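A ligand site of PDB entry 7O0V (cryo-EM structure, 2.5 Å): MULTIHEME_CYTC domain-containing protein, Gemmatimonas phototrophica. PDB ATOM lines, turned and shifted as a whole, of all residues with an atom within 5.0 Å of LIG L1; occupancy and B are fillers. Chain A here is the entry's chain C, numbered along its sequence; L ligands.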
ATOM      1  N   PRO A  63      -5.890 -11.427  -5.613  1.00  0.00           N
ATOM      2  CA  PRO A  63      -4.829 -10.592  -6.181  1.00  0.00           C
ATOM      3  C   PRO A  63      -5.272  -9.545  -7.200  1.00  0.00           C
ATOM      4  O   PRO A  63      -4.424  -8.761  -7.645  1.00  0.00           O
ATOM      5  CB  PRO A  63      -3.937 -11.645  -6.876  1.00  0.00           C
ATOM      6  CG  PRO A  63      -4.919 -12.645  -7.361  1.00  0.00           C
ATOM      7  CD  PRO A  63      -5.960 -12.746  -6.257  1.00  0.00           C
ATOM      8  N   TRP A  64      -6.540  -9.519  -7.584  1.00  0.00           N
ATOM      9  CA  TRP A  64      -6.962  -8.843  -8.812  1.00  0.00           C
ATOM     10  C   TRP A  64      -6.854  -7.325  -8.723  1.00  0.00           C
ATOM     11  O   TRP A  64      -7.032  -6.721  -7.661  1.00  0.00           O
ATOM     12  CB  TRP A  64      -8.405  -9.230  -9.140  1.00  0.00           C
ATOM     13  CG  TRP A  64      -8.709 -10.673  -8.962  1.00  0.00           C
ATOM     14  CD1 TRP A  64      -9.660 -11.211  -8.157  1.00  0.00           C
ATOM     15  CD2 TRP A  64      -8.084 -11.776  -9.642  1.00  0.00           C
ATOM     16  NE1 TRP A  64      -9.655 -12.583  -8.268  1.00  0.00           N
ATOM     17  CE2 TRP A  64      -8.702 -12.957  -9.178  1.00  0.00           C
ATOM     18  CE3 TRP A  64      -7.070 -11.884 -10.587  1.00  0.00           C
ATOM     19  CZ2 TRP A  64      -8.334 -14.217  -9.624  1.00  0.00           C
ATOM     20  CZ3 TRP A  64      -6.702 -13.144 -11.034  1.00  0.00           C
ATOM     21  CH2 TRP A  64      -7.330 -14.297 -10.548  1.00  0.00           C
ATOM     22  N   LYS A  65      -6.560  -6.720  -9.868  1.00  0.00           N
ATOM     23  CA  LYS A  65      -6.374  -5.287 -10.017  1.00  0.00           C
ATOM     24  C   LYS A  65      -7.620  -4.558 -10.490  1.00  0.00           C
ATOM     25  O   LYS A  65      -7.851  -3.416 -10.095  1.00  0.00           O
ATOM     26  CB  LYS A  65      -5.218  -5.003 -10.985  1.00  0.00           C
ATOM     27  CG  LYS A  65      -3.871  -5.408 -10.418  1.00  0.00           C
ATOM     28  CD  LYS A  65      -2.836  -5.655 -11.492  1.00  0.00           C
ATOM     29  CE  LYS A  65      -1.571  -6.246 -10.882  1.00  0.00           C
ATOM     30  NZ  LYS A  65      -0.618  -6.737 -11.913  1.00  0.00           N
ATOM     31  N   ASN A  66      -8.436  -5.201 -11.337  1.00  0.00           N
ATOM     32  CA  ASN A  66      -9.532  -4.526 -12.023  1.00  0.00           C
ATOM     33  C   ASN A  66     -10.701  -5.491 -12.162  1.00  0.00           C
ATOM     34  O   ASN A  66     -11.340  -5.585 -13.227  1.00  0.00           O
ATOM     35  CB  ASN A  66      -9.074  -4.002 -13.382  1.00  0.00           C
ATOM     36  CG  ASN A  66     -10.090  -3.073 -14.032  1.00  0.00           C
ATOM     37  OD1 ASN A  66     -10.932  -2.487 -13.348  1.00  0.00           O
ATOM     38  ND2 ASN A  66     -10.005  -2.926 -15.343  1.00  0.00           N
ATOM     39  N   VAL A  67     -11.003  -6.216 -11.089  1.00  0.00           N
ATOM     40  CA  VAL A  67     -12.157  -7.100 -10.992  1.00  0.00           C
ATOM     41  C   VAL A  67     -13.224  -6.423 -10.148  1.00  0.00           C
ATOM     42  O   VAL A  67     -12.955  -5.976  -9.024  1.00  0.00           O
ATOM     43  CB  VAL A  67     -11.776  -8.466 -10.413  1.00  0.00           C
ATOM     44  CG1 VAL A  67     -13.005  -9.227  -9.964  1.00  0.00           C
ATOM     45  CG2 VAL A  67     -11.019  -9.267 -11.458  1.00  0.00           C
ATOM     46  N   GLN A  68     -14.440  -6.347 -10.692  1.00  0.00           N
ATOM     47  CA  GLN A  68     -15.494  -5.493 -10.156  1.00  0.00           C
ATOM     48  C   GLN A  68     -16.798  -6.230  -9.916  1.00  0.00           C
ATOM     49  O   GLN A  68     -17.625  -5.750  -9.126  1.00  0.00           O
ATOM     50  CB  GLN A  68     -15.753  -4.316 -11.121  1.00  0.00           C
ATOM     51  CG  GLN A  68     -14.514  -3.477 -11.385  1.00  0.00           C
ATOM     52  CD  GLN A  68     -14.797  -2.231 -12.188  1.00  0.00           C
ATOM     53  OE1 GLN A  68     -15.434  -2.289 -13.230  1.00  0.00           O
ATOM     54  NE2 GLN A  68     -14.325  -1.086 -11.696  1.00  0.00           N
ATOM     55  N   VAL A  69     -17.008  -7.376 -10.557  1.00  0.00           N
ATOM     56  CA  VAL A  69     -18.200  -8.188 -10.384  1.00  0.00           C
ATOM     57  C   VAL A  69     -17.878  -9.482  -9.643  1.00  0.00           C
ATOM     58  O   VAL A  69     -18.540  -9.828  -8.667  1.00  0.00           O
ATOM     59  CB  VAL A  69     -18.868  -8.487 -11.750  1.00  0.00           C
ATOM     60  CG1 VAL A  69     -20.206  -9.176 -11.546  1.00  0.00           C
ATOM     61  CG2 VAL A  69     -19.043  -7.202 -12.547  1.00  0.00           C
ATOM     62  N   LEU A  70     -16.849 -10.187 -10.093  1.00  0.00           N
ATOM     63  CA  LEU A  70     -16.419 -11.479  -9.546  1.00  0.00           C
ATOM     64  C   LEU A  70     -15.582 -11.350  -8.273  1.00  0.00           C
ATOM     65  O   LEU A  70     -14.601 -12.074  -8.096  1.00  0.00           O
ATOM     66  CB  LEU A  70     -15.663 -12.247 -10.619  1.00  0.00           C
ATOM     67  CG  LEU A  70     -16.449 -12.520 -11.905  1.00  0.00           C
ATOM     68  CD1 LEU A  70     -15.627 -13.340 -12.884  1.00  0.00           C
ATOM     69  CD2 LEU A  70     -17.759 -13.225 -11.594  1.00  0.00           C
ATOM     70  N   PHE A  78     -12.533 -18.342 -10.062  1.00  0.00           N
ATOM     71  CA  PHE A  78     -12.366 -17.265 -11.044  1.00  0.00           C
ATOM     72  C   PHE A  78     -11.687 -17.768 -12.315  1.00  0.00           C
ATOM     73  O   PHE A  78     -12.169 -17.494 -13.417  1.00  0.00           O
ATOM     74  CB  PHE A  78     -11.566 -16.137 -10.382  1.00  0.00           C
ATOM     75  CG  PHE A  78     -11.419 -14.909 -11.229  1.00  0.00           C
ATOM     76  CD1 PHE A  78     -10.520 -14.866 -12.277  1.00  0.00           C
ATOM     77  CD2 PHE A  78     -12.169 -13.779 -10.951  1.00  0.00           C
ATOM     78  CE1 PHE A  78     -10.379 -13.721 -13.040  1.00  0.00           C
ATOM     79  CE2 PHE A  78     -12.034 -12.638 -11.708  1.00  0.00           C
ATOM     80  CZ  PHE A  78     -11.142 -12.611 -12.756  1.00  0.00           C
ATOM     81  N   MET A  82     -13.314 -17.995 -16.182  1.00  0.00           N
ATOM     82  CA  MET A  82     -12.751 -17.409 -17.408  1.00  0.00           C
ATOM     83  C   MET A  82     -12.559 -18.444 -18.510  1.00  0.00           C
ATOM     84  O   MET A  82     -12.732 -18.132 -19.696  1.00  0.00           O
ATOM     85  CB  MET A  82     -11.420 -16.730 -17.088  1.00  0.00           C
ATOM     86  CG  MET A  82     -11.545 -15.475 -16.248  1.00  0.00           C
ATOM     87  SD  MET A  82     -12.465 -14.169 -17.094  1.00  0.00           S
ATOM     88  CE  MET A  82     -13.042 -13.248 -15.678  1.00  0.00           C
ATOM     89  N   ILE A  83     -12.209 -19.680 -18.143  1.00  0.00           N
ATOM     90  CA  ILE A  83     -12.165 -20.753 -19.126  1.00  0.00           C
ATOM     91  C   ILE A  83     -13.548 -21.050 -19.690  1.00  0.00           C
ATOM     92  O   ILE A  83     -13.714 -21.300 -20.891  1.00  0.00           O
ATOM     93  CB  ILE A  83     -11.520 -22.013 -18.504  1.00  0.00           C
ATOM     94  CG1 ILE A  83     -10.048 -21.748 -18.184  1.00  0.00           C
ATOM     95  CG2 ILE A  83     -11.651 -23.197 -19.447  1.00  0.00           C
ATOM     96  CD1 ILE A  83      -9.480 -22.688 -17.151  1.00  0.00           C
ATOM     97  N   MET A  85     -16.187 -18.857 -19.847  1.00  0.00           N
ATOM     98  CA  MET A  85     -16.597 -17.730 -20.671  1.00  0.00           C
ATOM     99  C   MET A  85     -16.006 -17.800 -22.075  1.00  0.00           C
ATOM    100  O   MET A  85     -16.710 -17.619 -23.068  1.00  0.00           O
ATOM    101  CB  MET A  85     -16.202 -16.409 -20.026  1.00  0.00           C
ATOM    102  CG  MET A  85     -16.898 -16.077 -18.730  1.00  0.00           C
ATOM    103  SD  MET A  85     -16.516 -14.374 -18.292  1.00  0.00           S
ATOM    104  CE  MET A  85     -16.357 -14.490 -16.523  1.00  0.00           C
ATOM    105  N   SER A  86     -14.700 -18.041 -22.173  1.00  0.00           N
ATOM    106  CA  SER A  86     -14.067 -18.178 -23.483  1.00  0.00           C
ATOM    107  C   SER A  86     -14.677 -19.325 -24.271  1.00  0.00           C
ATOM    108  O   SER A  86     -14.957 -19.179 -25.472  1.00  0.00           O
ATOM    109  CB  SER A  86     -12.558 -18.356 -23.323  1.00  0.00           C
ATOM    110  OG  SER A  86     -12.266 -19.364 -22.368  1.00  0.00           O
ATOM    111  N   VAL A  89     -18.382 -18.093 -25.298  1.00  0.00           N
ATOM    112  CA  VAL A  89     -18.537 -16.924 -26.138  1.00  0.00           C
ATOM    113  C   VAL A  89     -17.549 -16.911 -27.296  1.00  0.00           C
ATOM    114  O   VAL A  89     -17.894 -16.478 -28.403  1.00  0.00           O
ATOM    115  CB  VAL A  89     -18.415 -15.630 -25.293  1.00  0.00           C
ATOM    116  CG1 VAL A  89     -18.686 -14.400 -26.153  1.00  0.00           C
ATOM    117  CG2 VAL A  89     -19.361 -15.675 -24.114  1.00  0.00           C
ATOM    118  N   ALA A  90     -16.326 -17.392 -27.082  1.00  0.00           N
ATOM    119  CA  ALA A  90     -15.212 -17.073 -27.967  1.00  0.00           C
ATOM    120  C   ALA A  90     -14.468 -18.279 -28.530  1.00  0.00           C
ATOM    121  O   ALA A  90     -13.632 -18.085 -29.423  1.00  0.00           O
ATOM    122  CB  ALA A  90     -14.210 -16.173 -27.235  1.00  0.00           C
ATOM    123  N   ASN A  94      -9.744 -18.768 -26.199  1.00  0.00           N
ATOM    124  CA  ASN A  94      -9.627 -17.474 -26.891  1.00  0.00           C
ATOM    125  C   ASN A  94      -9.713 -16.299 -25.922  1.00  0.00           C
ATOM    126  O   ASN A  94     -10.560 -15.415 -26.049  1.00  0.00           O
ATOM    127  CB  ASN A  94     -10.703 -17.393 -27.966  1.00  0.00           C
ATOM    128  CG  ASN A  94     -10.451 -16.291 -28.959  1.00  0.00           C
ATOM    129  OD1 ASN A  94      -9.400 -15.649 -28.943  1.00  0.00           O
ATOM    130  ND2 ASN A  94     -11.411 -16.059 -29.843  1.00  0.00           N
ATOM    131  N   CYS A  95      -8.817 -16.289 -24.925  1.00  0.00           N
ATOM    132  CA  CYS A  95      -8.767 -15.162 -23.986  1.00  0.00           C
ATOM    133  C   CYS A  95      -8.473 -13.848 -24.705  1.00  0.00           C
ATOM    134  O   CYS A  95      -8.844 -12.773 -24.197  1.00  0.00           O
ATOM    135  CB  CYS A  95      -7.707 -15.414 -22.914  1.00  0.00           C
ATOM    136  SG  CYS A  95      -7.842 -17.017 -22.079  1.00  0.00           S
ATOM    137  N   TYR A  97      -9.965 -12.743 -27.173  1.00  0.00           N
ATOM    138  CA  TYR A  97     -11.205 -12.113 -27.605  1.00  0.00           C
ATOM    139  C   TYR A  97     -11.569 -10.914 -26.727  1.00  0.00           C
ATOM    140  O   TYR A  97     -12.056  -9.897 -27.224  1.00  0.00           O
ATOM    141  CB  TYR A  97     -12.348 -13.119 -27.623  1.00  0.00           C
ATOM    142  CG  TYR A  97     -13.483 -12.642 -28.483  1.00  0.00           C
ATOM    143  CD1 TYR A  97     -13.454 -12.816 -29.858  1.00  0.00           C
ATOM    144  CD2 TYR A  97     -14.553 -11.947 -27.929  1.00  0.00           C
ATOM    145  CE1 TYR A  97     -14.501 -12.415 -30.644  1.00  0.00           C
ATOM    146  CE2 TYR A  97     -15.589 -11.493 -28.721  1.00  0.00           C
ATOM    147  CZ  TYR A  97     -15.562 -11.737 -30.076  1.00  0.00           C
ATOM    148  OH  TYR A  97     -16.546 -11.230 -30.879  1.00  0.00           O
ATOM    149  N   CYS A  98     -11.348 -11.024 -25.416  1.00  0.00           N
ATOM    150  CA  CYS A  98     -11.666  -9.937 -24.509  1.00  0.00           C
ATOM    151  C   CYS A  98     -10.454  -9.151 -24.024  1.00  0.00           C
ATOM    152  O   CYS A  98     -10.577  -7.960 -23.751  1.00  0.00           O
ATOM    153  CB  CYS A  98     -12.443 -10.462 -23.307  1.00  0.00           C
ATOM    154  SG  CYS A  98     -13.977 -11.318 -23.737  1.00  0.00           S
ATOM    155  N   HIS A  99      -9.294  -9.785 -23.908  1.00  0.00           N
ATOM    156  CA  HIS A  99      -8.177  -9.212 -23.168  1.00  0.00           C
ATOM    157  C   HIS A  99      -7.044  -8.767 -24.072  1.00  0.00           C
ATOM    158  O   HIS A  99      -6.830  -9.304 -25.166  1.00  0.00           O
ATOM    159  CB  HIS A  99      -7.615 -10.237 -22.186  1.00  0.00           C
ATOM    160  CG  HIS A  99      -8.500 -10.513 -21.014  1.00  0.00           C
ATOM    161  ND1 HIS A  99      -8.685  -9.625 -19.983  1.00  0.00           N
ATOM    162  CD2 HIS A  99      -9.243 -11.607 -20.695  1.00  0.00           C
ATOM    163  CE1 HIS A  99      -9.506 -10.144 -19.087  1.00  0.00           C
ATOM    164  NE2 HIS A  99      -9.855 -11.355 -19.496  1.00  0.00           N
ATOM    165  N   PHE A 104      -4.094  -8.746 -18.454  1.00  0.00           N
ATOM    166  CA  PHE A 104      -5.507  -9.074 -18.305  1.00  0.00           C
ATOM    167  C   PHE A 104      -6.312  -7.972 -17.619  1.00  0.00           C
ATOM    168  O   PHE A 104      -7.497  -7.804 -17.892  1.00  0.00           O
ATOM    169  CB  PHE A 104      -5.658 -10.387 -17.537  1.00  0.00           C
ATOM    170  CG  PHE A 104      -5.102 -11.577 -18.257  1.00  0.00           C
ATOM    171  CD1 PHE A 104      -5.759 -12.120 -19.343  1.00  0.00           C
ATOM    172  CD2 PHE A 104      -3.910 -12.153 -17.841  1.00  0.00           C
ATOM    173  CE1 PHE A 104      -5.245 -13.217 -20.007  1.00  0.00           C
ATOM    174  CE2 PHE A 104      -3.395 -13.250 -18.505  1.00  0.00           C
ATOM    175  CZ  PHE A 104      -4.063 -13.788 -19.584  1.00  0.00           C
ATOM    176  N   GLN A 105      -5.675  -7.223 -16.708  1.00  0.00           N
ATOM    177  CA  GLN A 105      -6.372  -6.138 -16.018  1.00  0.00           C
ATOM    178  C   GLN A 105      -6.709  -4.959 -16.923  1.00  0.00           C
ATOM    179  O   GLN A 105      -7.562  -4.141 -16.541  1.00  0.00           O
ATOM    180  CB  GLN A 105      -5.547  -5.670 -14.812  1.00  0.00           C
ATOM    181  CG  GLN A 105      -4.343  -4.783 -15.111  1.00  0.00           C
ATOM    182  CD  GLN A 105      -3.125  -5.575 -15.561  1.00  0.00           C
ATOM    183  OE1 GLN A 105      -3.231  -6.705 -16.035  1.00  0.00           O
ATOM    184  NE2 GLN A 105      -1.945  -4.973 -15.398  1.00  0.00           N
ATOM    185  N   THR A 117     -15.232  -5.502 -26.009  1.00  0.00           N
ATOM    186  CA  THR A 117     -15.732  -6.825 -25.640  1.00  0.00           C
ATOM    187  C   THR A 117     -15.582  -7.112 -24.150  1.00  0.00           C
ATOM    188  O   THR A 117     -16.472  -7.709 -23.542  1.00  0.00           O
ATOM    189  CB  THR A 117     -15.018  -7.913 -26.450  1.00  0.00           C
ATOM    190  OG1 THR A 117     -13.613  -7.623 -26.508  1.00  0.00           O
ATOM    191  CG2 THR A 117     -15.580  -7.967 -27.865  1.00  0.00           C
ATOM    192  N   LYS A 118     -14.463  -6.701 -23.540  1.00  0.00           N
ATOM    193  CA  LYS A 118     -14.344  -6.832 -22.085  1.00  0.00           C
ATOM    194  C   LYS A 118     -15.332  -5.927 -21.354  1.00  0.00           C
ATOM    195  O   LYS A 118     -15.879  -6.309 -20.316  1.00  0.00           O
ATOM    196  CB  LYS A 118     -12.910  -6.554 -21.646  1.00  0.00           C
ATOM    197  CG  LYS A 118     -12.669  -6.927 -20.189  1.00  0.00           C
ATOM    198  CD  LYS A 118     -11.274  -6.555 -19.736  1.00  0.00           C
ATOM    199  CE  LYS A 118     -11.105  -6.819 -18.245  1.00  0.00           C
ATOM    200  NZ  LYS A 118      -9.900  -6.140 -17.691  1.00  0.00           N
ATOM    201  N   ALA A 121     -18.636  -7.745 -21.711  1.00  0.00           N
ATOM    202  CA  ALA A 121     -18.647  -8.952 -20.886  1.00  0.00           C
ATOM    203  C   ALA A 121     -18.797  -8.662 -19.402  1.00  0.00           C
ATOM    204  O   ALA A 121     -19.457  -9.414 -18.686  1.00  0.00           O
ATOM    205  CB  ALA A 121     -17.375  -9.757 -21.142  1.00  0.00           C
ATOM    206  N   ARG A 122     -18.185  -7.575 -18.912  1.00  0.00           N
ATOM    207  CA  ARG A 122     -18.421  -7.185 -17.530  1.00  0.00           C
ATOM    208  C   ARG A 122     -19.888  -6.862 -17.276  1.00  0.00           C
ATOM    209  O   ARG A 122     -20.433  -7.220 -16.223  1.00  0.00           O
ATOM    210  CB  ARG A 122     -17.517  -6.012 -17.146  1.00  0.00           C
ATOM    211  CG  ARG A 122     -17.548  -5.687 -15.663  1.00  0.00           C
ATOM    212  CD  ARG A 122     -16.627  -4.528 -15.300  1.00  0.00           C
ATOM    213  NE  ARG A 122     -15.232  -4.935 -15.283  1.00  0.00           N
ATOM    214  CZ  ARG A 122     -14.233  -4.274 -15.871  1.00  0.00           C
ATOM    215  NH1 ARG A 122     -14.467  -3.254 -16.675  1.00  0.00           N
ATOM    216  NH2 ARG A 122     -12.991  -4.687 -15.677  1.00  0.00           N
ATOM    217  N   LEU A 125     -21.915 -10.166 -17.211  1.00  0.00           N
ATOM    218  CA  LEU A 125     -21.857 -10.843 -15.915  1.00  0.00           C
ATOM    219  C   LEU A 125     -22.913 -10.308 -14.959  1.00  0.00           C
ATOM    220  O   LEU A 125     -23.625 -11.091 -14.310  1.00  0.00           O
ATOM    221  CB  LEU A 125     -20.460 -10.699 -15.317  1.00  0.00           C
ATOM    222  CG  LEU A 125     -19.362 -11.597 -15.894  1.00  0.00           C
ATOM    223  CD1 LEU A 125     -17.998 -11.082 -15.498  1.00  0.00           C
ATOM    224  CD2 LEU A 125     -19.551 -13.016 -15.399  1.00  0.00           C
HETATM  225 FE1  LIG L   1     -11.019 -12.717 -18.359  1.00  0.00          FE
HETATM  226  C1  LIG L   1     -10.936 -10.430 -15.795  1.00  0.00           C
HETATM  227  C2  LIG L   1      -8.109 -14.117 -17.173  1.00  0.00           C
HETATM  228  C3  LIG L   1     -10.965 -14.925 -20.999  1.00  0.00           C
HETATM  229  C4  LIG L   1     -13.694 -11.149 -19.779  1.00  0.00           C
HETATM  230  N1  LIG L   1      -9.776 -12.360 -16.766  1.00  0.00           N
HETATM  231  C5  LIG L   1      -9.907 -11.327 -15.859  1.00  0.00           C
HETATM  232  C6  LIG L   1      -8.748 -11.351 -14.984  1.00  0.00           C
HETATM  233  C7  LIG L   1      -7.966 -12.371 -15.365  1.00  0.00           C
HETATM  234  C8  LIG L   1      -8.597 -13.027 -16.487  1.00  0.00           C
HETATM  235  C9  LIG L   1      -6.629 -12.780 -14.721  1.00  0.00           C
HETATM  236  C10 LIG L   1      -8.495 -10.370 -13.826  1.00  0.00           C
HETATM  237  C11 LIG L   1      -7.451  -9.323 -14.222  1.00  0.00           C
HETATM  238  C12 LIG L   1      -7.268  -8.360 -13.082  1.00  0.00           C
HETATM  239  O1  LIG L   1      -7.973  -7.312 -13.058  1.00  0.00           O
HETATM  240  O2  LIG L   1      -6.423  -8.634 -12.197  1.00  0.00           O
HETATM  241  N2  LIG L   1      -9.721 -14.181 -19.005  1.00  0.00           N
HETATM  242  C13 LIG L   1      -8.676 -14.701 -18.284  1.00  0.00           C
HETATM  243  C14 LIG L   1      -8.291 -15.964 -18.864  1.00  0.00           C
HETATM  244  C15 LIG L   1      -9.080 -16.179 -19.944  1.00  0.00           C
HETATM  245  C16 LIG L   1      -9.988 -15.065 -20.035  1.00  0.00           C
HETATM  246  C17 LIG L   1      -7.137 -16.826 -18.298  1.00  0.00           C
HETATM  247  C18 LIG L   1      -9.186 -17.327 -20.978  1.00  0.00           C
HETATM  248  C19 LIG L   1      -8.752 -18.733 -20.503  1.00  0.00           C
HETATM  249  N3  LIG L   1     -12.106 -12.996 -20.056  1.00  0.00           N
HETATM  250  C20 LIG L   1     -11.936 -13.962 -21.024  1.00  0.00           C
HETATM  251  C21 LIG L   1     -13.049 -13.900 -21.953  1.00  0.00           C
HETATM  252  C22 LIG L   1     -13.659 -12.724 -21.725  1.00  0.00           C
HETATM  253  C23 LIG L   1     -13.177 -12.222 -20.456  1.00  0.00           C
HETATM  254  C24 LIG L   1     -12.990 -14.668 -23.292  1.00  0.00           C
HETATM  255  C25 LIG L   1     -14.876 -12.039 -22.402  1.00  0.00           C
HETATM  256  C26 LIG L   1     -15.927 -13.010 -22.981  1.00  0.00           C
HETATM  257  N4  LIG L   1     -12.096 -11.011 -17.890  1.00  0.00           N
HETATM  258  C27 LIG L   1     -13.263 -10.666 -18.569  1.00  0.00           C
HETATM  259  C28 LIG L   1     -13.981  -9.696 -17.782  1.00  0.00           C
HETATM  260  C29 LIG L   1     -13.134  -9.468 -16.536  1.00  0.00           C
HETATM  261  C30 LIG L   1     -11.981 -10.317 -16.692  1.00  0.00           C
HETATM  262  C31 LIG L   1     -15.331  -9.024 -18.119  1.00  0.00           C
HETATM  263  C32 LIG L   1     -13.464  -8.512 -15.370  1.00  0.00           C
HETATM  264  C33 LIG L   1     -14.299  -9.245 -14.336  1.00  0.00           C
HETATM  265  C34 LIG L   1     -14.790  -8.268 -13.298  1.00  0.00           C
HETATM  266  O3  LIG L   1     -15.389  -8.727 -12.292  1.00  0.00           O
HETATM  267  O4  LIG L   1     -14.587  -7.045 -13.484  1.00  0.00           O
HETATM  268 FE1  LG2 L   2     -23.715 -11.639 -24.042  1.00  0.00          FE
HETATM  269  C1  LG2 L   2     -23.089  -9.558 -26.673  1.00  0.00           C
HETATM  270  C2  LG2 L   2     -20.343 -11.729 -23.312  1.00  0.00           C
HETATM  271  C3  LG2 L   2     -24.313 -13.833 -21.474  1.00  0.00           C
HETATM  272  C4  LG2 L   2     -27.055 -11.741 -24.829  1.00  0.00           C
HETATM  273  N1  LG2 L   2     -22.039 -10.787 -24.829  1.00  0.00           N
HETATM  274  C5  LG2 L   2     -22.000  -9.983 -25.949  1.00  0.00           C
HETATM  275  C6  LG2 L   2     -20.617  -9.662 -26.220  1.00  0.00           C
HETATM  276  C7  LG2 L   2     -19.867 -10.256 -25.301  1.00  0.00           C
HETATM  277  C8  LG2 L   2     -20.741 -10.979 -24.403  1.00  0.00           C
HETATM  278  C9  LG2 L   2     -18.322 -10.195 -25.199  1.00  0.00           C
HETATM  279  C10 LG2 L   2     -20.134  -8.775 -27.388  1.00  0.00           C
HETATM  280  C11 LG2 L   2     -19.960  -9.637 -28.638  1.00  0.00           C
HETATM  281  C12 LG2 L   2     -19.441  -8.799 -29.770  1.00  0.00           C
HETATM  282  O1  LG2 L   2     -18.676  -9.338 -30.606  1.00  0.00           O
HETATM  283  O2  LG2 L   2     -19.797  -7.597 -29.834  1.00  0.00           O
HETATM  284  N2  LG2 L   2     -22.535 -12.650 -22.698  1.00  0.00           N
HETATM  285  C13 LG2 L   2     -21.185 -12.446 -22.483  1.00  0.00           C
HETATM  286  C14 LG2 L   2     -20.825 -13.088 -21.236  1.00  0.00           C
HETATM  287  C15 LG2 L   2     -21.924 -13.693 -20.758  1.00  0.00           C
HETATM  288  C16 LG2 L   2     -23.011 -13.396 -21.654  1.00  0.00           C
HETATM  289  C17 LG2 L   2     -19.376 -13.088 -20.680  1.00  0.00           C
HETATM  290  C18 LG2 L   2     -22.198 -14.515 -19.473  1.00  0.00           C
HETATM  291  C19 LG2 L   2     -21.473 -14.023 -18.200  1.00  0.00           C
HETATM  292  N3  LG2 L   2     -25.352 -12.585 -23.282  1.00  0.00           N
HETATM  293  C20 LG2 L   2     -25.384 -13.479 -22.234  1.00  0.00           C
HETATM  294  C21 LG2 L   2     -26.774 -13.816 -21.949  1.00  0.00           C
HETATM  295  C22 LG2 L   2     -27.477 -13.404 -23.024  1.00  0.00           C
HETATM  296  C23 LG2 L   2     -26.640 -12.515 -23.780  1.00  0.00           C
HETATM  297  C24 LG2 L   2     -27.112 -14.991 -21.005  1.00  0.00           C
HETATM  298  C25 LG2 L   2     -28.987 -13.517 -23.358  1.00  0.00           C
HETATM  299  C26 LG2 L   2     -29.916 -13.425 -22.133  1.00  0.00           C
HETATM  300  N4  LG2 L   2     -24.876 -10.817 -25.543  1.00  0.00           N
HETATM  301  C27 LG2 L   2     -26.259 -10.922 -25.602  1.00  0.00           C
HETATM  302  C28 LG2 L   2     -26.763 -10.037 -26.618  1.00  0.00           C
HETATM  303  C29 LG2 L   2     -25.524  -9.353 -27.202  1.00  0.00           C
HETATM  304  C30 LG2 L   2     -24.402  -9.908 -26.471  1.00  0.00           C
HETATM  305  C31 LG2 L   2     -28.235  -9.829 -27.024  1.00  0.00           C
HETATM  306  C32 LG2 L   2     -25.452  -8.310 -28.324  1.00  0.00           C
HETATM  307  C33 LG2 L   2     -24.907  -9.039 -29.548  1.00  0.00           C
HETATM  308  C34 LG2 L   2     -24.218  -8.077 -30.465  1.00  0.00           C
HETATM  309  O3  LG2 L   2     -23.169  -7.512 -30.061  1.00  0.00           O
HETATM  310  O4  LG2 L   2     -24.711  -7.868 -31.596  1.00  0.00           O
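Trp 64 touches LIG L1.
Val 67 touches LIG L1.
CE1 of Phe 78 touches C6 of LIG L1, 3.5 Å away.
CA of Ser 86 touches C24 of LIG L1, at 3.7 Å.
Asn 94 touches LIG L1.
Phe 104 touches LIG L1.
Gln 105 touches LIG L1.
O of Lys 118 touches C31 of LIG L1, 3.5 Å away.
Ala 121 touches LIG L1 (CB to C25, 3.6 Å).
Hydrophobic or aromatic side chains within 4 Å of LIG L1: Trp 64, Val 67, Val 69, Leu 70, Phe 78, Met 82, His 99, Phe 104 and Ala 121.
19 residues have an atom within 4 Å of LIG L1: Trp 64, Lys 65, Asn 66, Val 67, Gln 68, Val 69, Leu 70, Phe 78, Met 82, Ser 86, Asn 94, Cys 95, Cys 98, His 99, Phe 104, Gln 105, Lys 118, Ala 121 and Arg 122.
A ring nitrogen (ND1) of His 99 sits at hydrogen-bond distance from the backbone carbonyl oxygen of Phe 104 (3.0 Å).
OG of Ser 86 sits at hydrogen-bond distance from O of Met 82 (3.0 Å).
The backbone carbonyl oxygen (O) of Asn 66 sits at hydrogen-bond distance from the guanidinium group (NH2) of Arg 122 (3.1 Å).
The side-chain amide nitrogen (ND2) of Asn 66 lies within hydrogen-bond range of the backbone carbonyl oxygen (O) of Gln 105 (3.0 Å).
The guanidinium group (NE) of Arg 122 lies close to the side-chain amide oxygen (OE1) of Gln 68 (3.4 Å).
NZ of Lys 118 lies within hydrogen-bond range of O of Gln 105 (3.3 Å).
The side-chain amino group (NZ) of Lys 118 lies within hydrogen-bond range of the backbone carbonyl oxygen (O) of Phe 104.
The backbone NH of Tyr 97 sits at hydrogen-bond distance from the side-chain amide oxygen of Asn 94 (3.4 Å).
The side-chain sulfur (SG) of Cys 98 is covalently linked to a carbon (C25) of LIG L1, 1.8 Å away.
SG of Cys 95 is covalently linked to C18 of LIG L1, 1.8 Å away.
FE1 of LIG L1 is bound by NE2 of His 99.
FE1 of LIG L1 is bound by SD of Met 82, 2.4 Å away.
N of Val 69 sits at hydrogen-bond distance from O3 of LIG L1, 2.7 Å away.
The backbone NH (N) of Asn 66 lies within hydrogen-bond range of an oxygen (O1) of LIG L1 (2.8 Å).
An oxygen (O4) of LIG L1 is in salt-bridge range of the guanidinium group (NE) of Arg 122, 2.8 Å away.
O4 of LIG L1 sits at hydrogen-bond distance from N of Gln 68, 2.9 Å away.
N of Leu 70 sits at hydrogen-bond distance from O3 of LIG L1 (3.0 Å).
The backbone NH (N) of Lys 65 is in hydrogen-bond range of an oxygen (O2) of LIG L1 (3.0 Å).
OH of Tyr 97 sits at hydrogen-bond distance from O1 of LG2 L2 (2.9 Å).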
